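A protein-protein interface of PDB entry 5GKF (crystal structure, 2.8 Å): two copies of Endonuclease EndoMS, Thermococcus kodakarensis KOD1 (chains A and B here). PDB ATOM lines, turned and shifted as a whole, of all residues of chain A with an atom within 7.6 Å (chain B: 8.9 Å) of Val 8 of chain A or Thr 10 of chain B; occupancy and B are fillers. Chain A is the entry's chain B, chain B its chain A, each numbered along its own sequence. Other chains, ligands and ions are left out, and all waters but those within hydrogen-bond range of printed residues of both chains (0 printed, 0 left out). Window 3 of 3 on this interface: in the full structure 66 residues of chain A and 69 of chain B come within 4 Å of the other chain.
Of the 16 printed residues of chain A, 7 touch a printed residue of chain B. Of the 17 printed residues of chain B, 6 touch a printed residue of chain A. Hydrophobic or aromatic side chains of chain B that line the printed part of chain A: Val 6, Phe 34, Tyr 113 and Met 114.
N of Ser 11 of chain B is in hydrogen-bond range of O of Tyr 113 of chain B (2.9 Å). The backbone NH (N) of Tyr 113 of chain B lies within hydrogen-bond range of the backbone carbonyl oxygen (O) of Phe 34 of chain B (3.0 Å). The backbone NH (N) of Phe 34 of chain B sits at hydrogen-bond distance from the backbone carbonyl oxygen (O) of Met 114 of chain B (3.1 Å). O of Thr 32 of chain A is in hydrogen-bond range of N of Ser 116 of chain A, at 2.9 Å. The backbone NH of Tyr 113 of chain A lies within hydrogen-bond range of the backbone carbonyl oxygen of Phe 34 of chain A, 2.8 Å away. N of Phe 34 of chain A lies within hydrogen-bond range of O of Met 114 of chain A, 2.9 Å away.
Val 8 of chain A touches Thr 10 of chain B, but with the chains exchanged Thr 10 of chain A does not touch Val 8 of chain B (4.1 Å). Thr 10 of chain A touches Val 6 of chain B, but with the chains exchanged Val 6 of chain A does not touch Thr 10 of chain B (4.4 Å). Phe 34 of chain A touches Val 6 of chain B, but with the chains exchanged Val 6 of chain A does not touch Phe 34 of chain B (4.1 Å). Phe 34 of chain A touches Ser 116 of chain B, and with the chains exchanged Ser 116 of chain A touches Phe 34 of chain B. Positions printed for both chains: 6, 7, 8, 9, 10, 12, 16, 20, 34, 113, 114, 115 and 116. Of the 9 pairs that touch across the chains among the printed residues, 4 have their exchanged pair printed and touching as well.
Among the printed residues, pairs that only touch across the chains: Val 6 of chain A with Tyr 113 of chain B (3.5 Å), Val 8 of chain A with Thr 10 of chain B (3.7 Å), Val 8 of chain A with Met 114 of chain B (3.9 Å), Thr 10 of chain A with Val 6 of chain B (3.95 Å), Thr 32 of chain A with Phe 34 of chain B (3.4 Å), Phe 34 of chain A with Val 6 of chain B (3.95 Å), Phe 34 of chain A with Ser 116 of chain B (3.5 Å), Tyr 113 of chain A with Val 6 of chain B (3.6 Å) and Ser 116 of chain A with Phe 34 of chain B (3.5 Å).
No residue of chain B comes within 4 Å of Thr 7 of chain A. Val 8 of chain A touches two residues of chain B. No residue of chain B comes within 4 Å of Ile 9 of chain A. Met 114 of chain A touches none of the printed residues of chain B. Printed residues of chain B within 4 Å of Ser 116 of chain A: Phe 34. Printed residues of chain A within 4 Å of Val 6 of chain B: Thr 10, Phe 34 and Tyr 113. Of chain A, only Val 8 (3.7 Å) comes within 4 Å of Thr 10 of chain B. Of the printed residues of chain A, Phe 34 of chain B touches Thr 32 (3.4 Å) and Ser 116 (3.5 Å). Of the printed residues of chain A, Tyr 113 of chain B touches Val 6. Val 115 of chain B touches none of the printed residues of chain A.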
ATOM      1  N   VAL A   6      20.044  22.921 -14.588  1.00  0.00           N
ATOM      2  CA  VAL A   6      18.936  22.858 -15.517  1.00  0.00           C
ATOM      3  C   VAL A   6      19.260  22.019 -16.737  1.00  0.00           C
ATOM      4  O   VAL A   6      20.355  22.093 -17.266  1.00  0.00           O
ATOM      5  CB  VAL A   6      18.522  24.272 -15.991  1.00  0.00           C
ATOM      6  CG1 VAL A   6      17.313  24.216 -16.928  1.00  0.00           C
ATOM      7  CG2 VAL A   6      18.220  25.148 -14.812  1.00  0.00           C
ATOM      8  N   THR A   7      18.281  21.234 -17.179  1.00  0.00           N
ATOM      9  CA  THR A   7      18.325  20.544 -18.451  1.00  0.00           C
ATOM     10  C   THR A   7      16.984  20.791 -19.162  1.00  0.00           C
ATOM     11  O   THR A   7      15.945  20.654 -18.548  1.00  0.00           O
ATOM     12  CB  THR A   7      18.605  19.037 -18.248  1.00  0.00           C
ATOM     13  OG1 THR A   7      19.751  18.870 -17.399  1.00  0.00           O
ATOM     14  CG2 THR A   7      18.861  18.368 -19.565  1.00  0.00           C
ATOM     15  N   VAL A   8      17.009  21.183 -20.436  1.00  0.00           N
ATOM     16  CA  VAL A   8      15.797  21.612 -21.147  1.00  0.00           C
ATOM     17  C   VAL A   8      15.731  21.065 -22.548  1.00  0.00           C
ATOM     18  O   VAL A   8      16.733  21.046 -23.246  1.00  0.00           O
ATOM     19  CB  VAL A   8      15.678  23.151 -21.342  1.00  0.00           C
ATOM     20  CG1 VAL A   8      14.237  23.522 -21.495  1.00  0.00           C
ATOM     21  CG2 VAL A   8      16.306  23.932 -20.232  1.00  0.00           C
ATOM     22  N   ILE A   9      14.548  20.659 -22.990  1.00  0.00           N
ATOM     23  CA  ILE A   9      14.414  20.257 -24.369  1.00  0.00           C
ATOM     24  C   ILE A   9      13.095  20.762 -24.895  1.00  0.00           C
ATOM     25  O   ILE A   9      12.059  20.515 -24.295  1.00  0.00           O
ATOM     26  CB  ILE A   9      14.495  18.736 -24.540  1.00  0.00           C
ATOM     27  CG1 ILE A   9      15.872  18.211 -24.153  1.00  0.00           C
ATOM     28  CG2 ILE A   9      14.227  18.343 -25.975  1.00  0.00           C
ATOM     29  CD1 ILE A   9      15.894  16.742 -24.143  1.00  0.00           C
ATOM     30  N   THR A  10      13.138  21.470 -26.020  1.00  0.00           N
ATOM     31  CA  THR A  10      11.928  21.888 -26.697  1.00  0.00           C
ATOM     32  C   THR A  10      11.628  20.884 -27.805  1.00  0.00           C
ATOM     33  O   THR A  10      12.538  20.265 -28.345  1.00  0.00           O
ATOM     34  CB  THR A  10      12.035  23.325 -27.216  1.00  0.00           C
ATOM     35  OG1 THR A  10      13.355  23.555 -27.692  1.00  0.00           O
ATOM     36  CG2 THR A  10      11.796  24.288 -26.069  1.00  0.00           C
ATOM     37  N   PRO A  12      10.599  17.767 -27.640  1.00  0.00           N
ATOM     38  CA  PRO A  12      11.405  16.561 -27.410  1.00  0.00           C
ATOM     39  C   PRO A  12      10.855  15.316 -28.113  1.00  0.00           C
ATOM     40  O   PRO A  12       9.659  15.172 -28.299  1.00  0.00           O
ATOM     41  CB  PRO A  12      11.362  16.398 -25.893  1.00  0.00           C
ATOM     42  CG  PRO A  12      10.122  17.084 -25.465  1.00  0.00           C
ATOM     43  CD  PRO A  12       9.764  18.120 -26.481  1.00  0.00           C
ATOM     44  N   GLU A  16      13.875  11.341 -25.704  1.00  0.00           N
ATOM     45  CA  GLU A  16      14.358  12.403 -24.842  1.00  0.00           C
ATOM     46  C   GLU A  16      13.401  12.693 -23.689  1.00  0.00           C
ATOM     47  O   GLU A  16      13.854  12.920 -22.569  1.00  0.00           O
ATOM     48  CB  GLU A  16      14.589  13.672 -25.647  1.00  0.00           C
ATOM     49  CG  GLU A  16      15.862  13.650 -26.405  1.00  0.00           C
ATOM     50  CD  GLU A  16      15.928  14.717 -27.466  1.00  0.00           C
ATOM     51  OE1 GLU A  16      14.864  15.041 -28.091  1.00  0.00           O
ATOM     52  OE2 GLU A  16      17.063  15.217 -27.656  1.00  0.00           O
ATOM     53  N   LEU A  20      14.411  12.428 -19.674  1.00  0.00           N
ATOM     54  CA  LEU A  20      14.422  13.498 -18.692  1.00  0.00           C
ATOM     55  C   LEU A  20      13.403  13.234 -17.590  1.00  0.00           C
ATOM     56  O   LEU A  20      13.729  13.256 -16.396  1.00  0.00           O
ATOM     57  CB  LEU A  20      14.135  14.840 -19.364  1.00  0.00           C
ATOM     58  CG  LEU A  20      15.235  15.409 -20.254  1.00  0.00           C
ATOM     59  CD1 LEU A  20      14.817  16.772 -20.710  1.00  0.00           C
ATOM     60  CD2 LEU A  20      16.502  15.486 -19.450  1.00  0.00           C
ATOM     61  N   THR A  32       9.499  20.121 -14.827  1.00  0.00           N
ATOM     62  CA  THR A  32       8.526  21.056 -15.390  1.00  0.00           C
ATOM     63  C   THR A  32       8.282  20.761 -16.861  1.00  0.00           C
ATOM     64  O   THR A  32       9.224  20.543 -17.611  1.00  0.00           O
ATOM     65  CB  THR A  32       8.988  22.530 -15.247  1.00  0.00           C
ATOM     66  OG1 THR A  32       9.410  22.778 -13.899  1.00  0.00           O
ATOM     67  CG2 THR A  32       7.870  23.526 -15.645  1.00  0.00           C
ATOM     68  N   PHE A  34       5.758  21.926 -20.442  1.00  0.00           N
ATOM     69  CA  PHE A  34       4.729  22.677 -21.133  1.00  0.00           C
ATOM     70  C   PHE A  34       4.190  21.769 -22.224  1.00  0.00           C
ATOM     71  O   PHE A  34       4.965  21.350 -23.088  1.00  0.00           O
ATOM     72  CB  PHE A  34       5.265  23.989 -21.747  1.00  0.00           C
ATOM     73  CG  PHE A  34       6.041  24.880 -20.788  1.00  0.00           C
ATOM     74  CD1 PHE A  34       6.984  25.776 -21.278  1.00  0.00           C
ATOM     75  CD2 PHE A  34       5.826  24.836 -19.413  1.00  0.00           C
ATOM     76  CE1 PHE A  34       7.713  26.593 -20.421  1.00  0.00           C
ATOM     77  CE2 PHE A  34       6.553  25.655 -18.539  1.00  0.00           C
ATOM     78  CZ  PHE A  34       7.501  26.532 -19.047  1.00  0.00           C
ATOM     79  N   TYR A 113       5.708  20.567 -25.633  1.00  0.00           N
ATOM     80  CA  TYR A 113       6.540  21.654 -26.162  1.00  0.00           C
ATOM     81  C   TYR A 113       7.848  21.757 -25.421  1.00  0.00           C
ATOM     82  O   TYR A 113       8.862  22.058 -26.028  1.00  0.00           O
ATOM     83  CB  TYR A 113       5.842  22.994 -26.080  1.00  0.00           C
ATOM     84  CG  TYR A 113       4.408  22.965 -26.511  1.00  0.00           C
ATOM     85  CD1 TYR A 113       4.085  22.888 -27.846  1.00  0.00           C
ATOM     86  CD2 TYR A 113       3.370  23.029 -25.578  1.00  0.00           C
ATOM     87  CE1 TYR A 113       2.781  22.855 -28.260  1.00  0.00           C
ATOM     88  CE2 TYR A 113       2.054  23.014 -25.991  1.00  0.00           C
ATOM     89  CZ  TYR A 113       1.779  22.930 -27.346  1.00  0.00           C
ATOM     90  OH  TYR A 113       0.501  22.924 -27.813  1.00  0.00           O
ATOM     91  N   MET A 114       7.819  21.536 -24.107  1.00  0.00           N
ATOM     92  CA  MET A 114       9.040  21.565 -23.327  1.00  0.00           C
ATOM     93  C   MET A 114       9.033  20.617 -22.145  1.00  0.00           C
ATOM     94  O   MET A 114       8.038  20.488 -21.448  1.00  0.00           O
ATOM     95  CB  MET A 114       9.306  22.980 -22.825  1.00  0.00           C
ATOM     96  CG  MET A 114      10.701  23.156 -22.274  1.00  0.00           C
ATOM     97  SD  MET A 114      10.751  24.060 -20.723  1.00  0.00           S
ATOM     98  CE  MET A 114       9.782  23.005 -19.648  1.00  0.00           C
ATOM     99  N   VAL A 115      10.164  19.969 -21.907  1.00  0.00           N
ATOM    100  CA  VAL A 115      10.379  19.208 -20.681  1.00  0.00           C
ATOM    101  C   VAL A 115      11.686  19.698 -20.073  1.00  0.00           C
ATOM    102  O   VAL A 115      12.586  20.117 -20.802  1.00  0.00           O
ATOM    103  CB  VAL A 115      10.416  17.677 -20.939  1.00  0.00           C
ATOM    104  CG1 VAL A 115      11.316  17.352 -22.136  1.00  0.00           C
ATOM    105  CG2 VAL A 115      10.827  16.893 -19.657  1.00  0.00           C
ATOM    106  N   SER A 116      11.773  19.697 -18.745  1.00  0.00           N
ATOM    107  CA  SER A 116      12.927  20.277 -18.070  1.00  0.00           C
ATOM    108  C   SER A 116      13.202  19.704 -16.672  1.00  0.00           C
ATOM    109  O   SER A 116      12.294  19.286 -15.951  1.00  0.00           O
ATOM    110  CB  SER A 116      12.753  21.782 -17.973  1.00  0.00           C
ATOM    111  OG  SER A 116      11.711  22.066 -17.070  1.00  0.00           O
ATOM    112  N   VAL A 117      14.472  19.690 -16.295  1.00  0.00           N
ATOM    113  CA  VAL A 117      14.863  19.179 -14.995  1.00  0.00           C
ATOM    114  C   VAL A 117      15.600  20.264 -14.252  1.00  0.00           C
ATOM    115  O   VAL A 117      16.585  20.814 -14.735  1.00  0.00           O
ATOM    116  CB  VAL A 117      15.738  17.953 -15.094  1.00  0.00           C
ATOM    117  CG1 VAL A 117      16.091  17.488 -13.719  1.00  0.00           C
ATOM    118  CG2 VAL A 117      15.012  16.853 -15.858  1.00  0.00           C
ATOM    119  N   ARG A 119      17.426  20.974 -10.809  1.00  0.00           N
ATOM    120  CA  ARG A 119      17.958  20.347  -9.611  1.00  0.00           C
ATOM    121  C   ARG A 119      18.196  21.468  -8.648  1.00  0.00           C
ATOM    122  O   ARG A 119      19.253  22.104  -8.648  1.00  0.00           O
ATOM    123  CB  ARG A 119      19.251  19.603  -9.919  1.00  0.00           C
ATOM    124  CG  ARG A 119      19.104  18.688 -11.107  1.00  0.00           C
ATOM    125  CD  ARG A 119      20.424  18.210 -11.691  1.00  0.00           C
ATOM    126  NE  ARG A 119      20.173  17.033 -12.522  1.00  0.00           N
ATOM    127  CZ  ARG A 119      19.891  17.069 -13.820  1.00  0.00           C
ATOM    128  NH1 ARG A 119      19.856  18.234 -14.480  1.00  0.00           N
ATOM    129  NH2 ARG A 119      19.665  15.925 -14.460  1.00  0.00           N
ATOM    130  N   VAL B   6       6.774  28.384 -27.529  1.00  0.00           N
ATOM    131  CA  VAL B   6       7.719  28.421 -26.408  1.00  0.00           C
ATOM    132  C   VAL B   6       9.034  29.088 -26.789  1.00  0.00           C
ATOM    133  O   VAL B   6       9.579  28.858 -27.858  1.00  0.00           O
ATOM    134  CB  VAL B   6       8.029  26.969 -25.839  1.00  0.00           C
ATOM    135  CG1 VAL B   6       9.185  26.990 -24.850  1.00  0.00           C
ATOM    136  CG2 VAL B   6       6.795  26.344 -25.187  1.00  0.00           C
ATOM    137  N   THR B   7       9.534  29.908 -25.875  1.00  0.00           N
ATOM    138  CA  THR B   7      10.895  30.444 -25.884  1.00  0.00           C
ATOM    139  C   THR B   7      11.677  30.059 -24.591  1.00  0.00           C
ATOM    140  O   THR B   7      11.159  30.197 -23.487  1.00  0.00           O
ATOM    141  CB  THR B   7      10.841  31.962 -26.012  1.00  0.00           C
ATOM    142  OG1 THR B   7       9.902  32.328 -27.044  1.00  0.00           O
ATOM    143  CG2 THR B   7      12.220  32.535 -26.266  1.00  0.00           C
ATOM    144  N   VAL B   8      12.902  29.558 -24.707  1.00  0.00           N
ATOM    145  CA  VAL B   8      13.698  29.238 -23.520  1.00  0.00           C
ATOM    146  C   VAL B   8      15.074  29.825 -23.672  1.00  0.00           C
ATOM    147  O   VAL B   8      15.724  29.611 -24.686  1.00  0.00           O
ATOM    148  CB  VAL B   8      13.880  27.698 -23.279  1.00  0.00           C
ATOM    149  CG1 VAL B   8      14.814  27.460 -22.123  1.00  0.00           C
ATOM    150  CG2 VAL B   8      12.580  26.989 -23.045  1.00  0.00           C
ATOM    151  N   ILE B   9      15.536  30.557 -22.675  1.00  0.00           N
ATOM    152  CA  ILE B   9      16.945  30.919 -22.632  1.00  0.00           C
ATOM    153  C   ILE B   9      17.546  30.555 -21.291  1.00  0.00           C
ATOM    154  O   ILE B   9      17.260  31.180 -20.284  1.00  0.00           O
ATOM    155  CB  ILE B   9      17.167  32.413 -22.851  1.00  0.00           C
ATOM    156  CG1 ILE B   9      16.410  32.897 -24.073  1.00  0.00           C
ATOM    157  CG2 ILE B   9      18.632  32.718 -22.979  1.00  0.00           C
ATOM    158  CD1 ILE B   9      16.530  34.340 -24.255  1.00  0.00           C
ATOM    159  N   THR B  10      18.413  29.565 -21.287  1.00  0.00           N
ATOM    160  CA  THR B  10      19.160  29.225 -20.098  1.00  0.00           C
ATOM    161  C   THR B  10      20.276  30.223 -19.900  1.00  0.00           C
ATOM    162  O   THR B  10      20.802  30.752 -20.875  1.00  0.00           O
ATOM    163  CB  THR B  10      19.760  27.835 -20.218  1.00  0.00           C
ATOM    164  OG1 THR B  10      20.512  27.780 -21.439  1.00  0.00           O
ATOM    165  CG2 THR B  10      18.655  26.774 -20.238  1.00  0.00           C
ATOM    166  N   SER B  11      20.656  30.422 -18.641  1.00  0.00           N
ATOM    167  CA  SER B  11      21.605  31.454 -18.190  1.00  0.00           C
ATOM    168  C   SER B  11      21.507  32.744 -18.968  1.00  0.00           C
ATOM    169  O   SER B  11      22.464  33.131 -19.624  1.00  0.00           O
ATOM    170  CB  SER B  11      23.045  30.946 -18.259  1.00  0.00           C
ATOM    171  OG  SER B  11      23.215  29.806 -17.437  1.00  0.00           O
ATOM    172  N   PRO B  12      20.353  33.417 -18.901  1.00  0.00           N
ATOM    173  CA  PRO B  12      20.194  34.580 -19.775  1.00  0.00           C
ATOM    174  C   PRO B  12      21.076  35.721 -19.312  1.00  0.00           C
ATOM    175  O   PRO B  12      21.558  35.681 -18.184  1.00  0.00           O
ATOM    176  CB  PRO B  12      18.709  34.922 -19.640  1.00  0.00           C
ATOM    177  CG  PRO B  12      18.315  34.401 -18.307  1.00  0.00           C
ATOM    178  CD  PRO B  12      19.185  33.209 -18.028  1.00  0.00           C
ATOM    179  N   SER B  13      21.320  36.696 -20.177  1.00  0.00           N
ATOM    180  CA  SER B  13      21.987  37.912 -19.750  1.00  0.00           C
ATOM    181  C   SER B  13      20.887  38.856 -19.339  1.00  0.00           C
ATOM    182  O   SER B  13      19.700  38.509 -19.453  1.00  0.00           O
ATOM    183  CB  SER B  13      22.834  38.516 -20.861  1.00  0.00           C
ATOM    184  OG  SER B  13      22.000  39.024 -21.891  1.00  0.00           O
ATOM    185  N   GLU B  16      18.557  39.781 -22.189  1.00  0.00           N
ATOM    186  CA  GLU B  16      17.760  38.605 -22.547  1.00  0.00           C
ATOM    187  C   GLU B  16      16.616  38.424 -21.541  1.00  0.00           C
ATOM    188  O   GLU B  16      15.456  38.258 -21.935  1.00  0.00           O
ATOM    189  CB  GLU B  16      18.625  37.331 -22.608  1.00  0.00           C
ATOM    190  CG  GLU B  16      19.917  37.468 -23.390  1.00  0.00           C
ATOM    191  CD  GLU B  16      20.611  36.138 -23.697  1.00  0.00           C
ATOM    192  OE1 GLU B  16      21.487  35.692 -22.916  1.00  0.00           O
ATOM    193  OE2 GLU B  16      20.307  35.548 -24.755  1.00  0.00           O
ATOM    194  N   LEU B  17      16.959  38.470 -20.249  1.00  0.00           N
ATOM    195  CA  LEU B  17      15.978  38.391 -19.160  1.00  0.00           C
ATOM    196  C   LEU B  17      14.868  39.411 -19.308  1.00  0.00           C
ATOM    197  O   LEU B  17      13.689  39.060 -19.274  1.00  0.00           O
ATOM    198  CB  LEU B  17      16.654  38.600 -17.804  1.00  0.00           C
ATOM    199  CG  LEU B  17      15.734  38.529 -16.577  1.00  0.00           C
ATOM    200  CD1 LEU B  17      14.962  37.227 -16.574  1.00  0.00           C
ATOM    201  CD2 LEU B  17      16.536  38.666 -15.274  1.00  0.00           C
ATOM    202  N   LEU B  20      12.633  38.906 -22.371  1.00  0.00           N
ATOM    203  CA  LEU B  20      11.665  37.816 -22.311  1.00  0.00           C
ATOM    204  C   LEU B  20      10.549  38.111 -21.355  1.00  0.00           C
ATOM    205  O   LEU B  20       9.383  37.945 -21.699  1.00  0.00           O
ATOM    206  CB  LEU B  20      12.322  36.499 -21.926  1.00  0.00           C
ATOM    207  CG  LEU B  20      12.873  35.676 -23.084  1.00  0.00           C
ATOM    208  CD1 LEU B  20      12.680  34.229 -22.719  1.00  0.00           C
ATOM    209  CD2 LEU B  20      12.165  36.021 -24.380  1.00  0.00           C
ATOM    210  N   PHE B  34      13.409  29.605 -13.611  1.00  0.00           N
ATOM    211  CA  PHE B  34      14.147  28.843 -12.598  1.00  0.00           C
ATOM    212  C   PHE B  34      15.266  29.756 -12.175  1.00  0.00           C
ATOM    213  O   PHE B  34      16.009  30.224 -13.017  1.00  0.00           O
ATOM    214  CB  PHE B  34      14.723  27.520 -13.116  1.00  0.00           C
ATOM    215  CG  PHE B  34      13.708  26.587 -13.752  1.00  0.00           C
ATOM    216  CD1 PHE B  34      14.130  25.576 -14.606  1.00  0.00           C
ATOM    217  CD2 PHE B  34      12.350  26.701 -13.485  1.00  0.00           C
ATOM    218  CE1 PHE B  34      13.223  24.725 -15.198  1.00  0.00           C
ATOM    219  CE2 PHE B  34      11.430  25.846 -14.072  1.00  0.00           C
ATOM    220  CZ  PHE B  34      11.866  24.861 -14.936  1.00  0.00           C
ATOM    221  N   VAL B 112      19.700  33.722 -12.543  1.00  0.00           N
ATOM    222  CA  VAL B 112      18.622  33.074 -13.267  1.00  0.00           C
ATOM    223  C   VAL B 112      19.147  31.953 -14.154  1.00  0.00           C
ATOM    224  O   VAL B 112      19.818  32.170 -15.152  1.00  0.00           O
ATOM    225  CB  VAL B 112      17.854  34.098 -14.119  1.00  0.00           C
ATOM    226  CG1 VAL B 112      16.800  33.427 -14.997  1.00  0.00           C
ATOM    227  CG2 VAL B 112      17.264  35.177 -13.218  1.00  0.00           C
ATOM    228  N   TYR B 113      18.822  30.735 -13.783  1.00  0.00           N
ATOM    229  CA  TYR B 113      19.240  29.588 -14.541  1.00  0.00           C
ATOM    230  C   TYR B 113      18.471  29.436 -15.840  1.00  0.00           C
ATOM    231  O   TYR B 113      18.998  28.904 -16.812  1.00  0.00           O
ATOM    232  CB  TYR B 113      19.065  28.326 -13.721  1.00  0.00           C
ATOM    233  CG  TYR B 113      19.606  28.393 -12.321  1.00  0.00           C
ATOM    234  CD1 TYR B 113      20.970  28.527 -12.079  1.00  0.00           C
ATOM    235  CD2 TYR B 113      18.749  28.293 -11.227  1.00  0.00           C
ATOM    236  CE1 TYR B 113      21.462  28.558 -10.776  1.00  0.00           C
ATOM    237  CE2 TYR B 113      19.232  28.332  -9.931  1.00  0.00           C
ATOM    238  CZ  TYR B 113      20.581  28.456  -9.710  1.00  0.00           C
ATOM    239  OH  TYR B 113      21.029  28.500  -8.416  1.00  0.00           O
ATOM    240  N   MET B 114      17.206  29.822 -15.847  1.00  0.00           N
ATOM    241  CA  MET B 114      16.394  29.646 -17.056  1.00  0.00           C
ATOM    242  C   MET B 114      15.235  30.606 -17.049  1.00  0.00           C
ATOM    243  O   MET B 114      14.753  30.986 -15.986  1.00  0.00           O
ATOM    244  CB  MET B 114      15.869  28.212 -17.177  1.00  0.00           C
ATOM    245  CG  MET B 114      15.325  27.861 -18.546  1.00  0.00           C
ATOM    246  SD  MET B 114      13.991  26.642 -18.544  1.00  0.00           S
ATOM    247  CE  MET B 114      12.683  27.664 -17.838  1.00  0.00           C
ATOM    248  N   VAL B 115      14.778  30.976 -18.238  1.00  0.00           N
ATOM    249  CA  VAL B 115      13.663  31.890 -18.377  1.00  0.00           C
ATOM    250  C   VAL B 115      12.901  31.440 -19.605  1.00  0.00           C
ATOM    251  O   VAL B 115      13.484  31.029 -20.601  1.00  0.00           O
ATOM    252  CB  VAL B 115      14.123  33.353 -18.490  1.00  0.00           C
ATOM    253  CG1 VAL B 115      15.098  33.499 -19.621  1.00  0.00           C
ATOM    254  CG2 VAL B 115      12.928  34.317 -18.666  1.00  0.00           C
ATOM    255  N   SER B 116      11.586  31.472 -19.512  1.00  0.00           N
ATOM    256  CA  SER B 116      10.775  30.916 -20.558  1.00  0.00           C
ATOM    257  C   SER B 116       9.431  31.608 -20.655  1.00  0.00           C
ATOM    258  O   SER B 116       8.853  32.074 -19.654  1.00  0.00           O
ATOM    259  CB  SER B 116      10.572  29.421 -20.338  1.00  0.00           C
ATOM    260  OG  SER B 116       9.749  29.181 -19.206  1.00  0.00           O
